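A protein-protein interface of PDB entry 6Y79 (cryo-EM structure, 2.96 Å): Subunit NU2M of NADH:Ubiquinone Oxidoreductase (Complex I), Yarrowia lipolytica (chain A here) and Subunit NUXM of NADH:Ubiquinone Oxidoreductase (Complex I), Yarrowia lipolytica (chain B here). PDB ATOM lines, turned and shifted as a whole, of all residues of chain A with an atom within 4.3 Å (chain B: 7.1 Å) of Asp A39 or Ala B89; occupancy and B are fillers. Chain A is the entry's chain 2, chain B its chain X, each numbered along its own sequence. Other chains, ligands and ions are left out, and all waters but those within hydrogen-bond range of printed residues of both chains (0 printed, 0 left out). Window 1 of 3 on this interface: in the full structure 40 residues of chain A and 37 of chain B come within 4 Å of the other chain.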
ATOM      1  N   MET A   1      32.624 -25.016   8.735  1.00  0.00           N
ATOM      2  CA  MET A   1      31.368 -24.712   9.398  1.00  0.00           C
ATOM      3  C   MET A   1      31.363 -25.166  10.841  1.00  0.00           C
ATOM      4  O   MET A   1      30.466 -24.825  11.599  1.00  0.00           O
ATOM      5  CB  MET A   1      30.209 -25.345   8.653  1.00  0.00           C
ATOM      6  CG  MET A   1      29.990 -24.714   7.311  1.00  0.00           C
ATOM      7  SD  MET A   1      28.355 -25.040   6.696  1.00  0.00           S
ATOM      8  CE  MET A   1      27.460 -24.158   7.949  1.00  0.00           C
ATOM      9  N   VAL A  35      23.951 -29.283   8.596  1.00  0.00           N
ATOM     10  CA  VAL A  35      25.202 -29.336   7.862  1.00  0.00           C
ATOM     11  C   VAL A  35      25.296 -30.669   7.126  1.00  0.00           C
ATOM     12  O   VAL A  35      25.864 -30.735   6.034  1.00  0.00           O
ATOM     13  CB  VAL A  35      26.379 -29.071   8.818  1.00  0.00           C
ATOM     14  CG1 VAL A  35      27.724 -29.199   8.126  1.00  0.00           C
ATOM     15  CG2 VAL A  35      26.251 -27.683   9.405  1.00  0.00           C
ATOM     16  N   LEU A  36      24.690 -31.737   7.659  1.00  0.00           N
ATOM     17  CA  LEU A  36      24.642 -32.989   6.906  1.00  0.00           C
ATOM     18  C   LEU A  36      23.721 -32.872   5.706  1.00  0.00           C
ATOM     19  O   LEU A  36      24.089 -33.239   4.589  1.00  0.00           O
ATOM     20  CB  LEU A  36      24.142 -34.145   7.759  1.00  0.00           C
ATOM     21  CG  LEU A  36      24.776 -34.848   8.935  1.00  0.00           C
ATOM     22  CD1 LEU A  36      23.812 -35.951   9.277  1.00  0.00           C
ATOM     23  CD2 LEU A  36      26.103 -35.391   8.563  1.00  0.00           C
ATOM     24  N   VAL A  37      22.501 -32.400   5.935  1.00  0.00           N
ATOM     25  CA  VAL A  37      21.458 -32.453   4.922  1.00  0.00           C
ATOM     26  C   VAL A  37      21.728 -31.456   3.809  1.00  0.00           C
ATOM     27  O   VAL A  37      21.754 -31.812   2.627  1.00  0.00           O
ATOM     28  CB  VAL A  37      20.090 -32.203   5.576  1.00  0.00           C
ATOM     29  CG1 VAL A  37      19.030 -32.007   4.522  1.00  0.00           C
ATOM     30  CG2 VAL A  37      19.736 -33.347   6.498  1.00  0.00           C
ATOM     31  N   LEU A  38      21.952 -30.199   4.167  1.00  0.00           N
ATOM     32  CA  LEU A  38      22.032 -29.149   3.170  1.00  0.00           C
ATOM     33  C   LEU A  38      23.392 -29.036   2.504  1.00  0.00           C
ATOM     34  O   LEU A  38      23.524 -28.226   1.589  1.00  0.00           O
ATOM     35  CB  LEU A  38      21.674 -27.804   3.786  1.00  0.00           C
ATOM     36  CG  LEU A  38      20.182 -27.617   4.003  1.00  0.00           C
ATOM     37  CD1 LEU A  38      19.935 -26.274   4.618  1.00  0.00           C
ATOM     38  CD2 LEU A  38      19.429 -27.758   2.696  1.00  0.00           C
ATOM     39  N   ASP A  39      24.402 -29.800   2.922  1.00  0.00           N
ATOM     40  CA  ASP A  39      25.755 -29.552   2.443  1.00  0.00           C
ATOM     41  C   ASP A  39      26.527 -30.784   2.001  1.00  0.00           C
ATOM     42  O   ASP A  39      27.727 -30.666   1.734  1.00  0.00           O
ATOM     43  CB  ASP A  39      26.581 -28.837   3.514  1.00  0.00           C
ATOM     44  CG  ASP A  39      26.371 -27.366   3.506  1.00  0.00           C
ATOM     45  OD1 ASP A  39      26.026 -26.854   2.431  1.00  0.00           O
ATOM     46  OD2 ASP A  39      26.573 -26.715   4.549  1.00  0.00           O
ATOM     47  N   SER A  40      25.893 -31.953   1.901  1.00  0.00           N
ATOM     48  CA  SER A  40      26.641 -33.163   1.584  1.00  0.00           C
ATOM     49  C   SER A  40      26.802 -33.371   0.085  1.00  0.00           C
ATOM     50  O   SER A  40      27.544 -34.270  -0.320  1.00  0.00           O
ATOM     51  CB  SER A  40      25.969 -34.381   2.226  1.00  0.00           C
ATOM     52  OG  SER A  40      24.689 -34.621   1.685  1.00  0.00           O
ATOM     53  N   PHE A  41      26.194 -32.509  -0.749  1.00  0.00           N
ATOM     54  CA  PHE A  41      26.257 -32.576  -2.212  1.00  0.00           C
ATOM     55  C   PHE A  41      27.677 -32.413  -2.758  1.00  0.00           C
ATOM     56  O   PHE A  41      27.950 -32.727  -3.923  1.00  0.00           O
ATOM     57  CB  PHE A  41      25.322 -31.539  -2.850  1.00  0.00           C
ATOM     58  CG  PHE A  41      25.613 -30.120  -2.457  1.00  0.00           C
ATOM     59  CD1 PHE A  41      25.011 -29.564  -1.350  1.00  0.00           C
ATOM     60  CD2 PHE A  41      26.472 -29.336  -3.204  1.00  0.00           C
ATOM     61  CE1 PHE A  41      25.281 -28.275  -0.983  1.00  0.00           C
ATOM     62  CE2 PHE A  41      26.746 -28.051  -2.835  1.00  0.00           C
ATOM     63  CZ  PHE A  41      26.147 -27.526  -1.719  1.00  0.00           C
ATOM     64  N   LEU A  42      28.593 -31.960  -1.901  1.00  0.00           N
ATOM     65  CA  LEU A  42      30.030 -31.948  -2.133  1.00  0.00           C
ATOM     66  C   LEU A  42      30.622 -33.323  -2.435  1.00  0.00           C
ATOM     67  O   LEU A  42      31.767 -33.381  -2.899  1.00  0.00           O
ATOM     68  CB  LEU A  42      30.728 -31.365  -0.912  1.00  0.00           C
ATOM     69  CG  LEU A  42      30.346 -29.939  -0.542  1.00  0.00           C
ATOM     70  CD1 LEU A  42      31.063 -29.523   0.730  1.00  0.00           C
ATOM     71  CD2 LEU A  42      30.676 -29.002  -1.680  1.00  0.00           C
ATOM     72  N   ASP B  39      19.189 -20.897  -5.412  1.00  0.00           N
ATOM     73  CA  ASP B  39      20.199 -20.767  -4.366  1.00  0.00           C
ATOM     74  C   ASP B  39      19.745 -19.812  -3.267  1.00  0.00           C
ATOM     75  O   ASP B  39      19.952 -20.079  -2.075  1.00  0.00           O
ATOM     76  CB  ASP B  39      21.515 -20.306  -4.978  1.00  0.00           C
ATOM     77  CG  ASP B  39      22.104 -21.332  -5.909  1.00  0.00           C
ATOM     78  OD1 ASP B  39      21.832 -22.529  -5.707  1.00  0.00           O
ATOM     79  OD2 ASP B  39      22.835 -20.955  -6.843  1.00  0.00           O
ATOM     80  N   VAL B  42      17.473 -21.710  -1.228  1.00  0.00           N
ATOM     81  CA  VAL B  42      18.187 -22.551  -0.267  1.00  0.00           C
ATOM     82  C   VAL B  42      18.601 -21.740   0.959  1.00  0.00           C
ATOM     83  O   VAL B  42      18.508 -22.221   2.100  1.00  0.00           O
ATOM     84  CB  VAL B  42      19.390 -23.224  -0.955  1.00  0.00           C
ATOM     85  CG1 VAL B  42      20.329 -23.862   0.043  1.00  0.00           C
ATOM     86  CG2 VAL B  42      18.903 -24.277  -1.923  1.00  0.00           C
ATOM     87  N   ILE B  43      19.028 -20.490   0.746  1.00  0.00           N
ATOM     88  CA  ILE B  43      19.372 -19.609   1.868  1.00  0.00           C
ATOM     89  C   ILE B  43      18.142 -19.332   2.727  1.00  0.00           C
ATOM     90  O   ILE B  43      18.201 -19.379   3.964  1.00  0.00           O
ATOM     91  CB  ILE B  43      20.001 -18.298   1.366  1.00  0.00           C
ATOM     92  CG1 ILE B  43      21.258 -18.570   0.557  1.00  0.00           C
ATOM     93  CG2 ILE B  43      20.373 -17.413   2.529  1.00  0.00           C
ATOM     94  CD1 ILE B  43      21.927 -17.324   0.033  1.00  0.00           C
ATOM     95  N   ALA B  46      17.215 -22.533   4.755  1.00  0.00           N
ATOM     96  CA  ALA B  46      18.034 -22.744   5.943  1.00  0.00           C
ATOM     97  C   ALA B  46      17.795 -21.690   7.008  1.00  0.00           C
ATOM     98  O   ALA B  46      17.904 -21.987   8.199  1.00  0.00           O
ATOM     99  CB  ALA B  46      19.509 -22.754   5.582  1.00  0.00           C
ATOM    100  N   PHE B  83      21.189 -18.429   8.504  1.00  0.00           N
ATOM    101  CA  PHE B  83      21.766 -17.698   7.386  1.00  0.00           C
ATOM    102  C   PHE B  83      23.196 -18.144   7.107  1.00  0.00           C
ATOM    103  O   PHE B  83      23.611 -18.171   5.944  1.00  0.00           O
ATOM    104  CB  PHE B  83      21.720 -16.194   7.633  1.00  0.00           C
ATOM    105  CG  PHE B  83      22.184 -15.397   6.462  1.00  0.00           C
ATOM    106  CD1 PHE B  83      21.394 -15.281   5.338  1.00  0.00           C
ATOM    107  CD2 PHE B  83      23.421 -14.790   6.471  1.00  0.00           C
ATOM    108  CE1 PHE B  83      21.826 -14.561   4.250  1.00  0.00           C
ATOM    109  CE2 PHE B  83      23.860 -14.073   5.385  1.00  0.00           C
ATOM    110  CZ  PHE B  83      23.059 -13.957   4.274  1.00  0.00           C
ATOM    111  N   ALA B  84      23.946 -18.524   8.146  1.00  0.00           N
ATOM    112  CA  ALA B  84      25.302 -19.039   7.937  1.00  0.00           C
ATOM    113  C   ALA B  84      25.298 -20.360   7.166  1.00  0.00           C
ATOM    114  O   ALA B  84      26.073 -20.536   6.214  1.00  0.00           O
ATOM    115  CB  ALA B  84      26.007 -19.205   9.279  1.00  0.00           C
ATOM    116  N   VAL B  85      24.417 -21.293   7.556  1.00  0.00           N
ATOM    117  CA  VAL B  85      24.282 -22.569   6.845  1.00  0.00           C
ATOM    118  C   VAL B  85      23.802 -22.348   5.416  1.00  0.00           C
ATOM    119  O   VAL B  85      24.321 -22.958   4.473  1.00  0.00           O
ATOM    120  CB  VAL B  85      23.338 -23.522   7.605  1.00  0.00           C
ATOM    121  CG1 VAL B  85      23.120 -24.813   6.833  1.00  0.00           C
ATOM    122  CG2 VAL B  85      23.891 -23.864   8.938  1.00  0.00           C
ATOM    123  N   GLY B  86      22.824 -21.458   5.228  1.00  0.00           N
ATOM    124  CA  GLY B  86      22.308 -21.206   3.896  1.00  0.00           C
ATOM    125  C   GLY B  86      23.308 -20.536   2.982  1.00  0.00           C
ATOM    126  O   GLY B  86      23.365 -20.841   1.790  1.00  0.00           O
ATOM    127  N   PHE B  87      24.137 -19.647   3.526  1.00  0.00           N
ATOM    128  CA  PHE B  87      25.146 -19.024   2.687  1.00  0.00           C
ATOM    129  C   PHE B  87      26.260 -20.000   2.344  1.00  0.00           C
ATOM    130  O   PHE B  87      26.776 -19.970   1.223  1.00  0.00           O
ATOM    131  CB  PHE B  87      25.721 -17.776   3.347  1.00  0.00           C
ATOM    132  CG  PHE B  87      26.736 -17.089   2.495  1.00  0.00           C
ATOM    133  CD1 PHE B  87      26.335 -16.346   1.403  1.00  0.00           C
ATOM    134  CD2 PHE B  87      28.092 -17.227   2.750  1.00  0.00           C
ATOM    135  CE1 PHE B  87      27.256 -15.734   0.600  1.00  0.00           C
ATOM    136  CE2 PHE B  87      29.015 -16.622   1.944  1.00  0.00           C
ATOM    137  CZ  PHE B  87      28.596 -15.874   0.871  1.00  0.00           C
ATOM    138  N   GLY B  88      26.653 -20.863   3.288  1.00  0.00           N
ATOM    139  CA  GLY B  88      27.626 -21.898   2.961  1.00  0.00           C
ATOM    140  C   GLY B  88      27.118 -22.858   1.903  1.00  0.00           C
ATOM    141  O   GLY B  88      27.846 -23.216   0.970  1.00  0.00           O
ATOM    142  N   ALA B  89      25.836 -23.221   1.995  1.00  0.00           N
ATOM    143  CA  ALA B  89      25.216 -24.099   1.011  1.00  0.00           C
ATOM    144  C   ALA B  89      25.121 -23.441  -0.354  1.00  0.00           C
ATOM    145  O   ALA B  89      25.405 -24.078  -1.371  1.00  0.00           O
ATOM    146  CB  ALA B  89      23.832 -24.524   1.493  1.00  0.00           C
ATOM    147  N   ALA B  90      24.739 -22.165  -0.400  1.00  0.00           N
ATOM    148  CA  ALA B  90      24.597 -21.488  -1.682  1.00  0.00           C
ATOM    149  C   ALA B  90      25.948 -21.214  -2.323  1.00  0.00           C
ATOM    150  O   ALA B  90      26.077 -21.318  -3.546  1.00  0.00           O
ATOM    151  CB  ALA B  90      23.817 -20.194  -1.509  1.00  0.00           C
ATOM    152  N   TYR B  91      26.964 -20.878  -1.518  1.00  0.00           N
ATOM    153  CA  TYR B  91      28.303 -20.681  -2.059  1.00  0.00           C
ATOM    154  C   TYR B  91      28.858 -21.980  -2.623  1.00  0.00           C
ATOM    155  O   TYR B  91      29.470 -21.981  -3.697  1.00  0.00           O
ATOM    156  CB  TYR B  91      29.238 -20.101  -0.988  1.00  0.00           C
ATOM    157  CG  TYR B  91      30.623 -19.742  -1.499  1.00  0.00           C
ATOM    158  CD1 TYR B  91      30.885 -18.499  -2.050  1.00  0.00           C
ATOM    159  CD2 TYR B  91      31.667 -20.647  -1.423  1.00  0.00           C
ATOM    160  CE1 TYR B  91      32.147 -18.184  -2.535  1.00  0.00           C
ATOM    161  CE2 TYR B  91      32.920 -20.349  -1.900  1.00  0.00           C
ATOM    162  CZ  TYR B  91      33.159 -19.117  -2.456  1.00  0.00           C
ATOM    163  OH  TYR B  91      34.418 -18.813  -2.918  1.00  0.00           O
ATOM    164  N   ALA B  92      28.620 -23.105  -1.938  1.00  0.00           N
ATOM    165  CA  ALA B  92      29.117 -24.380  -2.443  1.00  0.00           C
ATOM    166  C   ALA B  92      28.374 -24.817  -3.696  1.00  0.00           C
ATOM    167  O   ALA B  92      28.998 -25.304  -4.650  1.00  0.00           O
ATOM    168  CB  ALA B  92      29.016 -25.442  -1.356  1.00  0.00           C
ATOM    169  N   ARG B  93      27.045 -24.633  -3.708  1.00  0.00           N
ATOM    170  CA  ARG B  93      26.231 -24.925  -4.884  1.00  0.00           C
ATOM    171  C   ARG B  93      26.700 -24.135  -6.088  1.00  0.00           C
ATOM    172  O   ARG B  93      26.945 -24.704  -7.150  1.00  0.00           O
ATOM    173  CB  ARG B  93      24.764 -24.607  -4.608  1.00  0.00           C
ATOM    174  CG  ARG B  93      24.035 -25.667  -3.859  1.00  0.00           C
ATOM    175  CD  ARG B  93      22.639 -25.224  -3.501  1.00  0.00           C
ATOM    176  NE  ARG B  93      21.724 -25.389  -4.622  1.00  0.00           N
ATOM    177  CZ  ARG B  93      21.137 -26.537  -4.937  1.00  0.00           C
ATOM    178  NH1 ARG B  93      21.369 -27.630  -4.216  1.00  0.00           N
ATOM    179  NH2 ARG B  93      20.318 -26.599  -5.976  1.00  0.00           N
ATOM    180  N   SER B  94      26.879 -22.826  -5.919  1.00  0.00           N
ATOM    181  CA  SER B  94      27.288 -21.985  -7.031  1.00  0.00           C
ATOM    182  C   SER B  94      28.722 -22.265  -7.475  1.00  0.00           C
ATOM    183  O   SER B  94      28.998 -22.202  -8.672  1.00  0.00           O
ATOM    184  CB  SER B  94      27.101 -20.522  -6.655  1.00  0.00           C
ATOM    185  OG  SER B  94      27.386 -19.678  -7.750  1.00  0.00           O
ATOM    186  N   SER B  95      29.632 -22.613  -6.552  1.00  0.00           N
ATOM    187  CA  SER B  95      30.998 -22.972  -6.936  1.00  0.00           C
ATOM    188  C   SER B  95      31.049 -24.263  -7.743  1.00  0.00           C
ATOM    189  O   SER B  95      31.933 -24.426  -8.601  1.00  0.00           O
ATOM    190  CB  SER B  95      31.875 -23.124  -5.698  1.00  0.00           C
ATOM    191  OG  SER B  95      31.980 -21.917  -4.978  1.00  0.00           O
ATOM    192  N   LEU B 150      34.458 -27.500   3.218  1.00  0.00           N
ATOM    193  CA  LEU B 150      33.495 -26.559   3.774  1.00  0.00           C
ATOM    194  C   LEU B 150      32.977 -27.015   5.128  1.00  0.00           C
ATOM    195  O   LEU B 150      32.522 -26.185   5.918  1.00  0.00           O
ATOM    196  CB  LEU B 150      32.332 -26.377   2.791  1.00  0.00           C
ATOM    197  CG  LEU B 150      31.179 -25.405   3.071  1.00  0.00           C
ATOM    198  CD1 LEU B 150      30.814 -24.657   1.844  1.00  0.00           C
ATOM    199  CD2 LEU B 150      29.960 -26.153   3.550  1.00  0.00           C
ATOM    200  N   PHE B 151      33.057 -28.310   5.420  1.00  0.00           N
ATOM    201  CA  PHE B 151      32.572 -28.832   6.692  1.00  0.00           C
ATOM    202  C   PHE B 151      33.451 -28.386   7.848  1.00  0.00           C
ATOM    203  O   PHE B 151      32.955 -28.148   8.952  1.00  0.00           O
ATOM    204  CB  PHE B 151      32.528 -30.353   6.648  1.00  0.00           C
ATOM    205  CG  PHE B 151      31.474 -30.908   5.748  1.00  0.00           C
ATOM    206  CD1 PHE B 151      30.448 -30.125   5.255  1.00  0.00           C
ATOM    207  CD2 PHE B 151      31.513 -32.231   5.397  1.00  0.00           C
ATOM    208  CE1 PHE B 151      29.498 -30.660   4.424  1.00  0.00           C
ATOM    209  CE2 PHE B 151      30.567 -32.770   4.573  1.00  0.00           C
ATOM    210  CZ  PHE B 151      29.555 -31.984   4.085  1.00  0.00           C
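N of Met A1 lies within hydrogen-bond range of O of Phe B151.
O of Leu B150 is in hydrogen-bond range of N of Met A1 (3.1 Å).
The guanidinium group of Arg B93 is in salt-bridge range of the side-chain carboxylate of Asp B39 (3.1 Å).
Among the printed residues, pairs that only touch across the chains: Asp A39 with Ala B89 (3.2 Å), Asp A39 with Phe B151 (3.2 Å), Phe A41 with Arg B93 (3.5 Å), Phe A41 with Ala B89 (3.5 Å), Phe A41 with Ala B92 (3.6 Å), Asp A39 with Leu B150 (3.6 Å), Leu A38 with Ala B46 (3.7 Å), Met A1 with Val B85 (3.7 Å), Leu A38 with Ala B89 (3.7 Å), Leu A42 with Ala B92 (3.9 Å), Leu A42 with Leu B150 (3.97 Å) and Val A35 with Phe B151 (3.98 Å).
Printed residues of chain B within 4 Å of Met A1: Val B85 (3.7 Å), Leu B150 (3.1 Å) and Phe B151 (3.2 Å).
Val B42 touches none of the printed residues of chain A.
Of the printed residues of chain A, Val B85 touches Met A1 (3.7 Å).
Printed residues of chain A within 4 Å of Ala B89: Leu A38 (3.7 Å), Asp A39 (3.2 Å) and Phe A41 (3.5 Å).
Printed residues of chain A within 4 Å of Ala B92: Phe A41 (3.6 Å) and Leu A42 (3.9 Å).
Of the printed residues of chain A, Leu B150 touches Met A1 (3.1 Å), Asp A39 (3.6 Å) and Leu A42 (3.97 Å).
Printed residues of chain A within 4 Å of Phe B151: Met A1 (3.2 Å), Val A35 (3.98 Å) and Asp A39 (3.2 Å).
The nearest printed residue of chain A that does not touch Ala B89 is Met A1 (5.6 Å).
The nearest printed residue of chain A that does not touch Leu B150 is Val A35 (5.9 Å).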
